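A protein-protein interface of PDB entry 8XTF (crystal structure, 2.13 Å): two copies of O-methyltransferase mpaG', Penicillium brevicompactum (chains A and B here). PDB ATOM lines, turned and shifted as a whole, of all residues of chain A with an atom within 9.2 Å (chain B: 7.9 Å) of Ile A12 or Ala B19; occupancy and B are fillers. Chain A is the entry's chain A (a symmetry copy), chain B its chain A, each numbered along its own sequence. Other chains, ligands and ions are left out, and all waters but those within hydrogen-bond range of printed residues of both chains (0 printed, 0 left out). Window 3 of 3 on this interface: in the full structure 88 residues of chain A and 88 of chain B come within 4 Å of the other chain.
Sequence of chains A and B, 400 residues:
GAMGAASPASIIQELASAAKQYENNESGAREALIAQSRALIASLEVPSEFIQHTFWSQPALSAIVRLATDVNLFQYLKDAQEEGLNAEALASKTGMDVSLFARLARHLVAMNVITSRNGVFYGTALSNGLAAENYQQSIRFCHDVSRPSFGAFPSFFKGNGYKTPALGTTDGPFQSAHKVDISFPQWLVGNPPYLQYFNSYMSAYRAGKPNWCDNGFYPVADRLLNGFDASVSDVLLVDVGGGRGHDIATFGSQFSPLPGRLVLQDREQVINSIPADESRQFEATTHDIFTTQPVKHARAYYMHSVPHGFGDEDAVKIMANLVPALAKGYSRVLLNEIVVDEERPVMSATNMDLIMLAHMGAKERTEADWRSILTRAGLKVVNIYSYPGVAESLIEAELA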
ATOM      1  N   ALA A   6     -25.664   4.971  17.627  1.00  0.00           N
ATOM      2  CA  ALA A   6     -24.554   4.525  16.791  1.00  0.00           C
ATOM      3  C   ALA A   6     -25.029   3.427  15.850  1.00  0.00           C
ATOM      4  O   ALA A   6     -25.687   2.474  16.277  1.00  0.00           O
ATOM      5  CB  ALA A   6     -23.391   4.026  17.648  1.00  0.00           C
ATOM      6  N   SER A   7     -24.705   3.574  14.567  1.00  0.00           N
ATOM      7  CA  SER A   7     -25.045   2.567  13.580  1.00  0.00           C
ATOM      8  C   SER A   7     -24.214   1.303  13.799  1.00  0.00           C
ATOM      9  O   SER A   7     -23.161   1.345  14.443  1.00  0.00           O
ATOM     10  CB  SER A   7     -24.814   3.112  12.172  1.00  0.00           C
ATOM     11  OG  SER A   7     -23.433   3.124  11.856  1.00  0.00           O
ATOM     12  N   PRO A   8     -24.678   0.158  13.292  1.00  0.00           N
ATOM     13  CA  PRO A   8     -23.825  -1.044  13.324  1.00  0.00           C
ATOM     14  C   PRO A   8     -22.487  -0.852  12.627  1.00  0.00           C
ATOM     15  O   PRO A   8     -21.480  -1.416  13.077  1.00  0.00           O
ATOM     16  CB  PRO A   8     -24.685  -2.105  12.617  1.00  0.00           C
ATOM     17  CG  PRO A   8     -26.074  -1.652  12.800  1.00  0.00           C
ATOM     18  CD  PRO A   8     -26.034  -0.135  12.806  1.00  0.00           C
ATOM     19  N   ALA A   9     -22.448  -0.072  11.544  1.00  0.00           N
ATOM     20  CA  ALA A   9     -21.196   0.164  10.829  1.00  0.00           C
ATOM     21  C   ALA A   9     -20.140   0.756  11.749  1.00  0.00           C
ATOM     22  O   ALA A   9     -19.002   0.277  11.801  1.00  0.00           O
ATOM     23  CB  ALA A   9     -21.438   1.087   9.636  1.00  0.00           C
ATOM     24  N   SER A  10     -20.504   1.798  12.494  1.00  0.00           N
ATOM     25  CA  SER A  10     -19.526   2.416  13.374  1.00  0.00           C
ATOM     26  C   SER A  10     -19.152   1.495  14.529  1.00  0.00           C
ATOM     27  O   SER A  10     -17.998   1.508  14.977  1.00  0.00           O
ATOM     28  CB  SER A  10     -20.054   3.758  13.891  1.00  0.00           C
ATOM     29  OG  SER A  10     -21.135   3.577  14.785  1.00  0.00           O
ATOM     30  N   ILE A  11     -20.098   0.677  15.011  1.00  0.00           N
ATOM     31  CA  ILE A  11     -19.795  -0.229  16.113  1.00  0.00           C
ATOM     32  C   ILE A  11     -18.872  -1.349  15.647  1.00  0.00           C
ATOM     33  O   ILE A  11     -18.017  -1.817  16.410  1.00  0.00           O
ATOM     34  CB  ILE A  11     -21.095  -0.783  16.731  1.00  0.00           C
ATOM     35  CG1 ILE A  11     -21.872   0.329  17.443  1.00  0.00           C
ATOM     36  CG2 ILE A  11     -20.790  -1.898  17.731  1.00  0.00           C
ATOM     37  CD1 ILE A  11     -23.335  -0.027  17.733  1.00  0.00           C
ATOM     38  N   ILE A  12     -19.022  -1.792  14.396  1.00  0.00           N
ATOM     39  CA  ILE A  12     -18.100  -2.772  13.822  1.00  0.00           C
ATOM     40  C   ILE A  12     -16.678  -2.219  13.806  1.00  0.00           C
ATOM     41  O   ILE A  12     -15.714  -2.931  14.114  1.00  0.00           O
ATOM     42  CB  ILE A  12     -18.578  -3.182  12.413  1.00  0.00           C
ATOM     43  CG1 ILE A  12     -19.780  -4.131  12.513  1.00  0.00           C
ATOM     44  CG2 ILE A  12     -17.447  -3.833  11.620  1.00  0.00           C
ATOM     45  CD1 ILE A  12     -20.710  -4.122  11.292  1.00  0.00           C
ATOM     46  N   GLN A  13     -16.530  -0.933  13.465  1.00  0.00           N
ATOM     47  CA  GLN A  13     -15.217  -0.293  13.477  1.00  0.00           C
ATOM     48  C   GLN A  13     -14.662  -0.197  14.894  1.00  0.00           C
ATOM     49  O   GLN A  13     -13.489  -0.516  15.130  1.00  0.00           O
ATOM     50  CB  GLN A  13     -15.300   1.097  12.840  1.00  0.00           C
ATOM     51  CG  GLN A  13     -15.643   1.090  11.352  1.00  0.00           C
ATOM     52  CD  GLN A  13     -15.989   2.477  10.816  1.00  0.00           C
ATOM     53  OE1 GLN A  13     -15.755   3.493  11.481  1.00  0.00           O
ATOM     54  NE2 GLN A  13     -16.563   2.520   9.608  1.00  0.00           N
ATOM     55  N   GLU A  14     -15.484   0.255  15.844  1.00  0.00           N
ATOM     56  CA  GLU A  14     -15.044   0.313  17.236  1.00  0.00           C
ATOM     57  C   GLU A  14     -14.645  -1.067  17.734  1.00  0.00           C
ATOM     58  O   GLU A  14     -13.657  -1.216  18.463  1.00  0.00           O
ATOM     59  CB  GLU A  14     -16.147   0.899  18.116  1.00  0.00           C
ATOM     60  CG  GLU A  14     -16.299   2.403  18.005  1.00  0.00           C
ATOM     61  CD  GLU A  14     -15.133   3.164  18.629  1.00  0.00           C
ATOM     62  OE1 GLU A  14     -14.070   3.286  17.973  1.00  0.00           O
ATOM     63  OE2 GLU A  14     -15.281   3.636  19.781  1.00  0.00           O
ATOM     64  N   LEU A  15     -15.395  -2.093  17.332  1.00  0.00           N
ATOM     65  CA  LEU A  15     -15.062  -3.449  17.739  1.00  0.00           C
ATOM     66  C   LEU A  15     -13.707  -3.873  17.181  1.00  0.00           C
ATOM     67  O   LEU A  15     -12.882  -4.432  17.914  1.00  0.00           O
ATOM     68  CB  LEU A  15     -16.168  -4.403  17.297  1.00  0.00           C
ATOM     69  CG  LEU A  15     -16.159  -5.759  17.982  1.00  0.00           C
ATOM     70  CD1 LEU A  15     -17.565  -6.232  18.201  1.00  0.00           C
ATOM     71  CD2 LEU A  15     -15.376  -6.744  17.120  1.00  0.00           C
ATOM     72  N   ALA A  16     -13.455  -3.608  15.887  1.00  0.00           N
ATOM     73  CA  ALA A  16     -12.147  -3.899  15.304  1.00  0.00           C
ATOM     74  C   ALA A  16     -11.028  -3.143  16.011  1.00  0.00           C
ATOM     75  O   ALA A  16      -9.913  -3.665  16.144  1.00  0.00           O
ATOM     76  CB  ALA A  16     -12.135  -3.555  13.817  1.00  0.00           C
ATOM     77  N   SER A  17     -11.293  -1.909  16.452  1.00  0.00           N
ATOM     78  CA  SER A  17     -10.263  -1.152  17.154  1.00  0.00           C
ATOM     79  C   SER A  17      -9.975  -1.765  18.522  1.00  0.00           C
ATOM     80  O   SER A  17      -8.814  -1.853  18.937  1.00  0.00           O
ATOM     81  CB  SER A  17     -10.683   0.311  17.279  1.00  0.00           C
ATOM     82  OG  SER A  17     -10.161   0.901  18.459  1.00  0.00           O
ATOM     83  N   ALA A  18     -11.013  -2.222  19.223  1.00  0.00           N
ATOM     84  CA  ALA A  18     -10.787  -2.854  20.516  1.00  0.00           C
ATOM     85  C   ALA A  18     -10.067  -4.187  20.371  1.00  0.00           C
ATOM     86  O   ALA A  18      -9.307  -4.574  21.262  1.00  0.00           O
ATOM     87  CB  ALA A  18     -12.111  -3.042  21.250  1.00  0.00           C
ATOM     88  N   ALA A  19     -10.270  -4.889  19.252  1.00  0.00           N
ATOM     89  CA  ALA A  19      -9.594  -6.167  19.063  1.00  0.00           C
ATOM     90  C   ALA A  19      -8.093  -5.971  18.922  1.00  0.00           C
ATOM     91  O   ALA A  19      -7.309  -6.796  19.402  1.00  0.00           O
ATOM     92  CB  ALA A  19     -10.161  -6.897  17.847  1.00  0.00           C
ATOM     93  N   LEU A  33     -13.781  -5.056  24.515  1.00  0.00           N
ATOM     94  CA  LEU A  33     -14.183  -5.892  23.390  1.00  0.00           C
ATOM     95  C   LEU A  33     -15.530  -6.569  23.658  1.00  0.00           C
ATOM     96  O   LEU A  33     -16.376  -6.665  22.758  1.00  0.00           O
ATOM     97  CB  LEU A  33     -13.095  -6.934  23.122  1.00  0.00           C
ATOM     98  CG  LEU A  33     -13.071  -7.684  21.797  1.00  0.00           C
ATOM     99  CD1 LEU A  33     -13.302  -6.725  20.654  1.00  0.00           C
ATOM    100  CD2 LEU A  33     -11.721  -8.359  21.657  1.00  0.00           C
ATOM    101  N   GLN A  36     -18.277  -3.805  23.328  1.00  0.00           N
ATOM    102  CA  GLN A  36     -18.609  -3.508  21.941  1.00  0.00           C
ATOM    103  C   GLN A  36     -19.443  -4.623  21.328  1.00  0.00           C
ATOM    104  O   GLN A  36     -20.344  -4.356  20.523  1.00  0.00           O
ATOM    105  CB  GLN A  36     -17.337  -3.296  21.120  1.00  0.00           C
ATOM    106  CG  GLN A  36     -16.616  -1.999  21.431  1.00  0.00           C
ATOM    107  CD  GLN A  36     -17.543  -0.796  21.381  1.00  0.00           C
ATOM    108  OE1 GLN A  36     -18.320  -0.628  20.435  1.00  0.00           O
ATOM    109  NE2 GLN A  36     -17.482   0.036  22.413  1.00  0.00           N
ATOM    110  N   SER A  37     -19.167  -5.874  21.697  1.00  0.00           N
ATOM    111  CA  SER A  37     -19.961  -6.959  21.133  1.00  0.00           C
ATOM    112  C   SER A  37     -21.415  -6.852  21.570  1.00  0.00           C
ATOM    113  O   SER A  37     -22.325  -7.097  20.771  1.00  0.00           O
ATOM    114  CB  SER A  37     -19.382  -8.313  21.525  1.00  0.00           C
ATOM    115  OG  SER A  37     -18.042  -8.429  21.091  1.00  0.00           O
ATOM    116  N   ALA A  39     -23.014  -4.109  22.450  1.00  0.00           N
ATOM    117  CA  ALA A  39     -23.591  -2.986  21.723  1.00  0.00           C
ATOM    118  C   ALA A  39     -23.918  -3.381  20.295  1.00  0.00           C
ATOM    119  O   ALA A  39     -24.961  -2.983  19.756  1.00  0.00           O
ATOM    120  CB  ALA A  39     -22.636  -1.796  21.744  1.00  0.00           C
ATOM    121  N   LEU A  40     -23.037  -4.165  19.662  1.00  0.00           N
ATOM    122  CA  LEU A  40     -23.294  -4.594  18.295  1.00  0.00           C
ATOM    123  C   LEU A  40     -24.568  -5.425  18.226  1.00  0.00           C
ATOM    124  O   LEU A  40     -25.445  -5.156  17.399  1.00  0.00           O
ATOM    125  CB  LEU A  40     -22.106  -5.376  17.733  1.00  0.00           C
ATOM    126  CG  LEU A  40     -22.298  -5.770  16.256  1.00  0.00           C
ATOM    127  CD1 LEU A  40     -22.577  -4.548  15.407  1.00  0.00           C
ATOM    128  CD2 LEU A  40     -21.115  -6.538  15.695  1.00  0.00           C
ATOM    129  N   ILE A  41     -24.690  -6.422  19.104  1.00  0.00           N
ATOM    130  CA  ILE A  41     -25.911  -7.216  19.177  1.00  0.00           C
ATOM    131  C   ILE A  41     -27.131  -6.320  19.337  1.00  0.00           C
ATOM    132  O   ILE A  41     -28.136  -6.485  18.634  1.00  0.00           O
ATOM    133  CB  ILE A  41     -25.819  -8.229  20.321  1.00  0.00           C
ATOM    134  CG1 ILE A  41     -24.783  -9.284  19.969  1.00  0.00           C
ATOM    135  CG2 ILE A  41     -27.177  -8.849  20.560  1.00  0.00           C
ATOM    136  CD1 ILE A  41     -24.263 -10.036  21.158  1.00  0.00           C
ATOM    137  N   SER A  43     -27.586  -3.298  18.468  1.00  0.00           N
ATOM    138  CA  SER A  43     -27.843  -2.495  17.276  1.00  0.00           C
ATOM    139  C   SER A  43     -28.389  -3.308  16.107  1.00  0.00           C
ATOM    140  O   SER A  43     -28.881  -2.717  15.141  1.00  0.00           O
ATOM    141  CB  SER A  43     -26.565  -1.785  16.821  1.00  0.00           C
ATOM    142  OG  SER A  43     -25.691  -2.680  16.148  1.00  0.00           O
ATOM    143  N   LEU A  44     -28.297  -4.631  16.153  1.00  0.00           N
ATOM    144  CA  LEU A  44     -28.765  -5.471  15.061  1.00  0.00           C
ATOM    145  C   LEU A  44     -30.059  -6.213  15.361  1.00  0.00           C
ATOM    146  O   LEU A  44     -30.801  -6.527  14.430  1.00  0.00           O
ATOM    147  CB  LEU A  44     -27.695  -6.499  14.692  1.00  0.00           C
ATOM    148  CG  LEU A  44     -26.348  -5.970  14.210  1.00  0.00           C
ATOM    149  CD1 LEU A  44     -25.348  -7.101  14.244  1.00  0.00           C
ATOM    150  CD2 LEU A  44     -26.449  -5.394  12.807  1.00  0.00           C
ATOM    151  N   ILE B  12     -12.799 -13.112  15.963  1.00  0.00           N
ATOM    152  CA  ILE B  12     -12.726 -11.730  15.491  1.00  0.00           C
ATOM    153  C   ILE B  12     -12.682 -11.690  13.965  1.00  0.00           C
ATOM    154  O   ILE B  12     -13.335 -10.853  13.330  1.00  0.00           O
ATOM    155  CB  ILE B  12     -11.509 -11.022  16.123  1.00  0.00           C
ATOM    156  CG1 ILE B  12     -11.798 -10.676  17.590  1.00  0.00           C
ATOM    157  CG2 ILE B  12     -11.140  -9.764  15.340  1.00  0.00           C
ATOM    158  CD1 ILE B  12     -10.554 -10.557  18.480  1.00  0.00           C
ATOM    159  N   GLN B  13     -11.925 -12.610  13.355  1.00  0.00           N
ATOM    160  CA  GLN B  13     -11.863 -12.695  11.899  1.00  0.00           C
ATOM    161  C   GLN B  13     -13.207 -13.111  11.311  1.00  0.00           C
ATOM    162  O   GLN B  13     -13.679 -12.508  10.337  1.00  0.00           O
ATOM    163  CB  GLN B  13     -10.767 -13.676  11.471  1.00  0.00           C
ATOM    164  CG  GLN B  13      -9.351 -13.236  11.830  1.00  0.00           C
ATOM    165  CD  GLN B  13      -8.318 -14.345  11.645  1.00  0.00           C
ATOM    166  OE1 GLN B  13      -8.600 -15.380  11.030  1.00  0.00           O
ATOM    167  NE2 GLN B  13      -7.115 -14.134  12.193  1.00  0.00           N
ATOM    168  N   GLU B  14     -13.830 -14.146  11.879  1.00  0.00           N
ATOM    169  CA  GLU B  14     -15.151 -14.561  11.414  1.00  0.00           C
ATOM    170  C   GLU B  14     -16.152 -13.424  11.548  1.00  0.00           C
ATOM    171  O   GLU B  14     -16.997 -13.218  10.670  1.00  0.00           O
ATOM    172  CB  GLU B  14     -15.628 -15.786  12.193  1.00  0.00           C
ATOM    173  CG  GLU B  14     -14.970 -17.085  11.775  1.00  0.00           C
ATOM    174  CD  GLU B  14     -15.416 -17.555  10.392  1.00  0.00           C
ATOM    175  OE1 GLU B  14     -14.890 -17.034   9.378  1.00  0.00           O
ATOM    176  OE2 GLU B  14     -16.298 -18.443  10.324  1.00  0.00           O
ATOM    177  N   LEU B  15     -16.057 -12.662  12.638  1.00  0.00           N
ATOM    178  CA  LEU B  15     -16.956 -11.535  12.826  1.00  0.00           C
ATOM    179  C   LEU B  15     -16.750 -10.481  11.745  1.00  0.00           C
ATOM    180  O   LEU B  15     -17.726  -9.984  11.170  1.00  0.00           O
ATOM    181  CB  LEU B  15     -16.756 -10.948  14.220  1.00  0.00           C
ATOM    182  CG  LEU B  15     -17.876 -10.041  14.703  1.00  0.00           C
ATOM    183  CD1 LEU B  15     -18.081 -10.219  16.177  1.00  0.00           C
ATOM    184  CD2 LEU B  15     -17.520  -8.595  14.369  1.00  0.00           C
ATOM    185  N   ALA B  16     -15.486 -10.133  11.446  1.00  0.00           N
ATOM    186  CA  ALA B  16     -15.204  -9.199  10.356  1.00  0.00           C
ATOM    187  C   ALA B  16     -15.723  -9.713   9.018  1.00  0.00           C
ATOM    188  O   ALA B  16     -16.164  -8.918   8.176  1.00  0.00           O
ATOM    189  CB  ALA B  16     -13.705  -8.932  10.255  1.00  0.00           C
ATOM    190  N   SER B  17     -15.660 -11.028   8.790  1.00  0.00           N
ATOM    191  CA  SER B  17     -16.162 -11.571   7.534  1.00  0.00           C
ATOM    192  C   SER B  17     -17.682 -11.458   7.461  1.00  0.00           C
ATOM    193  O   SER B  17     -18.237 -11.124   6.407  1.00  0.00           O
ATOM    194  CB  SER B  17     -15.708 -13.021   7.372  1.00  0.00           C
ATOM    195  OG  SER B  17     -16.653 -13.780   6.636  1.00  0.00           O
ATOM    196  N   ALA B  18     -18.373 -11.699   8.576  1.00  0.00           N
ATOM    197  CA  ALA B  18     -19.824 -11.562   8.570  1.00  0.00           C
ATOM    198  C   ALA B  18     -20.250 -10.110   8.406  1.00  0.00           C
ATOM    199  O   ALA B  18     -21.303  -9.841   7.823  1.00  0.00           O
ATOM    200  CB  ALA B  18     -20.415 -12.147   9.848  1.00  0.00           C
ATOM    201  N   ALA B  19     -19.439  -9.162   8.885  1.00  0.00           N
ATOM    202  CA  ALA B  19     -19.799  -7.756   8.742  1.00  0.00           C
ATOM    203  C   ALA B  19     -19.776  -7.335   7.283  1.00  0.00           C
ATOM    204  O   ALA B  19     -20.608  -6.531   6.852  1.00  0.00           O
ATOM    205  CB  ALA B  19     -18.865  -6.878   9.573  1.00  0.00           C
ATOM    206  N   LYS B  20     -18.837  -7.882   6.504  1.00  0.00           N
ATOM    207  CA  LYS B  20     -18.817  -7.620   5.067  1.00  0.00           C
ATOM    208  C   LYS B  20     -20.062  -8.174   4.391  1.00  0.00           C
ATOM    209  O   LYS B  20     -20.685  -7.493   3.567  1.00  0.00           O
ATOM    210  CB  LYS B  20     -17.561  -8.222   4.440  1.00  0.00           C
ATOM    211  CG  LYS B  20     -16.301  -7.425   4.701  1.00  0.00           C
ATOM    212  CD  LYS B  20     -16.536  -5.931   4.525  1.00  0.00           C
ATOM    213  CE  LYS B  20     -15.541  -5.334   3.539  1.00  0.00           C
ATOM    214  NZ  LYS B  20     -16.079  -4.131   2.845  1.00  0.00           N
ATOM    215  N   GLN B  21     -20.442  -9.410   4.728  1.00  0.00           N
ATOM    216  CA  GLN B  21     -21.670  -9.986   4.188  1.00  0.00           C
ATOM    217  C   GLN B  21     -22.899  -9.203   4.620  1.00  0.00           C
ATOM    218  O   GLN B  21     -23.848  -9.072   3.840  1.00  0.00           O
ATOM    219  CB  GLN B  21     -21.784 -11.446   4.609  1.00  0.00           C
ATOM    220  CG  GLN B  21     -20.513 -12.224   4.313  1.00  0.00           C
ATOM    221  CD  GLN B  21     -20.533 -13.623   4.883  1.00  0.00           C
ATOM    222  OE1 GLN B  21     -20.784 -13.817   6.067  1.00  0.00           O
ATOM    223  NE2 GLN B  21     -20.246 -14.604   4.046  1.00  0.00           N
ATOM    224  N   TYR B  22     -22.897  -8.661   5.840  1.00  0.00           N
ATOM    225  CA  TYR B  22     -24.011  -7.831   6.288  1.00  0.00           C
ATOM    226  C   TYR B  22     -24.055  -6.507   5.533  1.00  0.00           C
ATOM    227  O   TYR B  22     -25.137  -6.019   5.188  1.00  0.00           O
ATOM    228  CB  TYR B  22     -23.905  -7.587   7.791  1.00  0.00           C
ATOM    229  CG  TYR B  22     -24.881  -6.564   8.330  1.00  0.00           C
ATOM    230  CD1 TYR B  22     -26.231  -6.864   8.471  1.00  0.00           C
ATOM    231  CD2 TYR B  22     -24.451  -5.291   8.692  1.00  0.00           C
ATOM    232  CE1 TYR B  22     -27.124  -5.922   8.971  1.00  0.00           C
ATOM    233  CE2 TYR B  22     -25.329  -4.352   9.186  1.00  0.00           C
ATOM    234  CZ  TYR B  22     -26.662  -4.673   9.327  1.00  0.00           C
ATOM    235  OH  TYR B  22     -27.541  -3.737   9.820  1.00  0.00           O
ATOM    236  N   GLU B  23     -22.893  -5.912   5.264  1.00  0.00           N
ATOM    237  CA  GLU B  23     -22.869  -4.689   4.471  1.00  0.00           C
ATOM    238  C   GLU B  23     -23.343  -4.931   3.043  1.00  0.00           C
ATOM    239  O   GLU B  23     -24.008  -4.067   2.461  1.00  0.00           O
ATOM    240  CB  GLU B  23     -21.465  -4.085   4.481  1.00  0.00           C
ATOM    241  CG  GLU B  23     -21.160  -3.302   5.756  1.00  0.00           C
ATOM    242  CD  GLU B  23     -22.301  -2.363   6.158  1.00  0.00           C
ATOM    243  OE1 GLU B  23     -22.455  -1.300   5.512  1.00  0.00           O
ATOM    244  OE2 GLU B  23     -23.039  -2.683   7.122  1.00  0.00           O
ATOM    245  N   ASN B  24     -23.040  -6.101   2.474  1.00  0.00           N
ATOM    246  CA  ASN B  24     -23.493  -6.466   1.135  1.00  0.00           C
ATOM    247  C   ASN B  24     -24.941  -6.967   1.122  1.00  0.00           C
ATOM    248  O   ASN B  24     -25.459  -7.309   0.055  1.00  0.00           O
ATOM    249  CB  ASN B  24     -22.535  -7.516   0.547  1.00  0.00           C
ATOM    250  CG  ASN B  24     -22.808  -7.813  -0.915  1.00  0.00           C
ATOM    251  OD1 ASN B  24     -22.586  -8.933  -1.391  1.00  0.00           O
ATOM    252  ND2 ASN B  24     -23.300  -6.812  -1.637  1.00  0.00           N
ATOM    253  N   ASN B  25     -25.603  -7.008   2.282  1.00  0.00           N
ATOM    254  CA  ASN B  25     -27.029  -7.331   2.395  1.00  0.00           C
ATOM    255  C   ASN B  25     -27.321  -8.780   2.016  1.00  0.00           C
ATOM    256  O   ASN B  25     -28.357  -9.085   1.425  1.00  0.00           O
ATOM    257  CB  ASN B  25     -27.892  -6.377   1.570  1.00  0.00           C
ATOM    258  CG  ASN B  25     -27.955  -5.000   2.176  1.00  0.00           C
ATOM    259  OD1 ASN B  25     -28.511  -4.816   3.263  1.00  0.00           O
ATOM    260  ND2 ASN B  25     -27.372  -4.019   1.489  1.00  0.00           N
ATOM    261  N   ALA B  29     -27.176 -12.607   7.045  1.00  0.00           N
ATOM    262  CA  ALA B  29     -25.917 -12.064   7.541  1.00  0.00           C
ATOM    263  C   ALA B  29     -26.108 -11.291   8.838  1.00  0.00           C
ATOM    264  O   ALA B  29     -25.210 -11.284   9.685  1.00  0.00           O
ATOM    265  CB  ALA B  29     -25.264 -11.179   6.482  1.00  0.00           C
ATOM    266  N   ALA B  32     -26.143 -13.939  11.483  1.00  0.00           N
ATOM    267  CA  ALA B  32     -24.794 -14.491  11.612  1.00  0.00           C
ATOM    268  C   ALA B  32     -23.864 -13.541  12.356  1.00  0.00           C
ATOM    269  O   ALA B  32     -23.041 -13.978  13.166  1.00  0.00           O
ATOM    270  CB  ALA B  32     -24.225 -14.796  10.233  1.00  0.00           C
ATOM    271  N   LEU B  33     -23.960 -12.242  12.067  1.00  0.00           N
ATOM    272  CA  LEU B  33     -23.169 -11.248  12.781  1.00  0.00           C
ATOM    273  C   LEU B  33     -23.499 -11.249  14.277  1.00  0.00           C
ATOM    274  O   LEU B  33     -22.599 -11.131  15.120  1.00  0.00           O
ATOM    275  CB  LEU B  33     -23.419  -9.868  12.170  1.00  0.00           C
ATOM    276  CG  LEU B  33     -22.462  -8.721  12.463  1.00  0.00           C
ATOM    277  CD1 LEU B  33     -21.034  -9.197  12.348  1.00  0.00           C
ATOM    278  CD2 LEU B  33     -22.733  -7.610  11.468  1.00  0.00           C
ATOM    279  N   GLN B  36     -21.883 -14.471  15.795  1.00  0.00           N
ATOM    280  CA  GLN B  36     -20.451 -14.323  16.029  1.00  0.00           C
ATOM    281  C   GLN B  36     -20.183 -13.437  17.234  1.00  0.00           C
ATOM    282  O   GLN B  36     -19.235 -13.684  17.990  1.00  0.00           O
ATOM    283  CB  GLN B  36     -19.767 -13.744  14.791  1.00  0.00           C
ATOM    284  CG  GLN B  36     -19.678 -14.714  13.628  1.00  0.00           C
ATOM    285  CD  GLN B  36     -19.093 -16.055  14.038  1.00  0.00           C
ATOM    286  OE1 GLN B  36     -18.064 -16.121  14.720  1.00  0.00           O
ATOM    287  NE2 GLN B  36     -19.760 -17.131  13.644  1.00  0.00           N
ATOM    288  N   SER B  37     -21.003 -12.407  17.438  1.00  0.00           N
ATOM    289  CA  SER B  37     -20.774 -11.549  18.594  1.00  0.00           C
ATOM    290  C   SER B  37     -20.969 -12.322  19.891  1.00  0.00           C
ATOM    291  O   SER B  37     -20.207 -12.137  20.847  1.00  0.00           O
ATOM    292  CB  SER B  37     -21.689 -10.331  18.555  1.00  0.00           C
ATOM    293  OG  SER B  37     -21.486  -9.591  17.367  1.00  0.00           O
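Printed residues of chain B that touch a printed residue of chain A: Ile B12, Leu B15, Ala B19, Tyr B22, Leu B33 and Ser B37. Hydrophobic or aromatic side chains of chain B that line the printed part of chain A: Ile B12, Leu B15, Ala B19, Tyr B22 and Leu B33. Of the 22 printed residues of chain A, 8 touch a printed residue of chain B. Hydrophobic or aromatic side chains of chain A that line the printed part of chain B: Pro A8, Ile A12, Leu A15, Ala A19, Leu A40, Ile A41 and Leu A44.
CG of Pro A8 touches OH of Tyr B22, 3.9 Å away. CB of Ala B19 touches CD1 of Ile A12, 3.7 Å away. CD2 of Leu B15 touches CD2 of Leu A15, 3.9 Å away. CB of Ala A19 touches CD1 of Ile B12, at 3.7 Å. O of Ser B37 touches CB of Ser A37, at 3.97 Å. Ser B37 touches Leu A40 (OG to CD2, 3.5 Å). CG1 of Ile A41 touches CB of Ser B37 (3.6 Å). Leu A44 touches Tyr B22. Leu B33 touches Leu A44 (CG to CD1, 3.8 Å).
Ile A12 touches Ala B19, and with the chains exchanged Ala A19 touches Ile B12. Leu A15 touches its own counterpart, Leu B15. Ser A37 touches its own counterpart, Ser B37.
O of Leu B33 sits at hydrogen-bond distance from OG of Ser B37, 2.9 Å away. The side-chain hydroxyl (OG) of Ser A37 lies within hydrogen-bond range of the backbone carbonyl oxygen (O) of Leu A33 (2.9 Å). The backbone carbonyl oxygen of Leu A40 lies within hydrogen-bond range of the side-chain hydroxyl of Ser A43 (2.8 Å).
Of chain B, only Ala B19 comes within 4 Å of Ile A12. Ala B19 touches just one residue of chain A: Ile A12. Of the printed residues of chain B, Ile A41 touches Ser B37 (3.6 Å). Printed residues of chain A within 4 Å of Leu B15: Leu A15 (3.9 Å). Of the printed residues of chain B, Leu A40 touches Ser B37 (3.5 Å). Printed residues of chain B within 4 Å of Ser A37: Ser B37. Of the printed residues of chain A, Leu B33 touches Leu A44. Ala B29 touches none of the printed residues of chain A.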
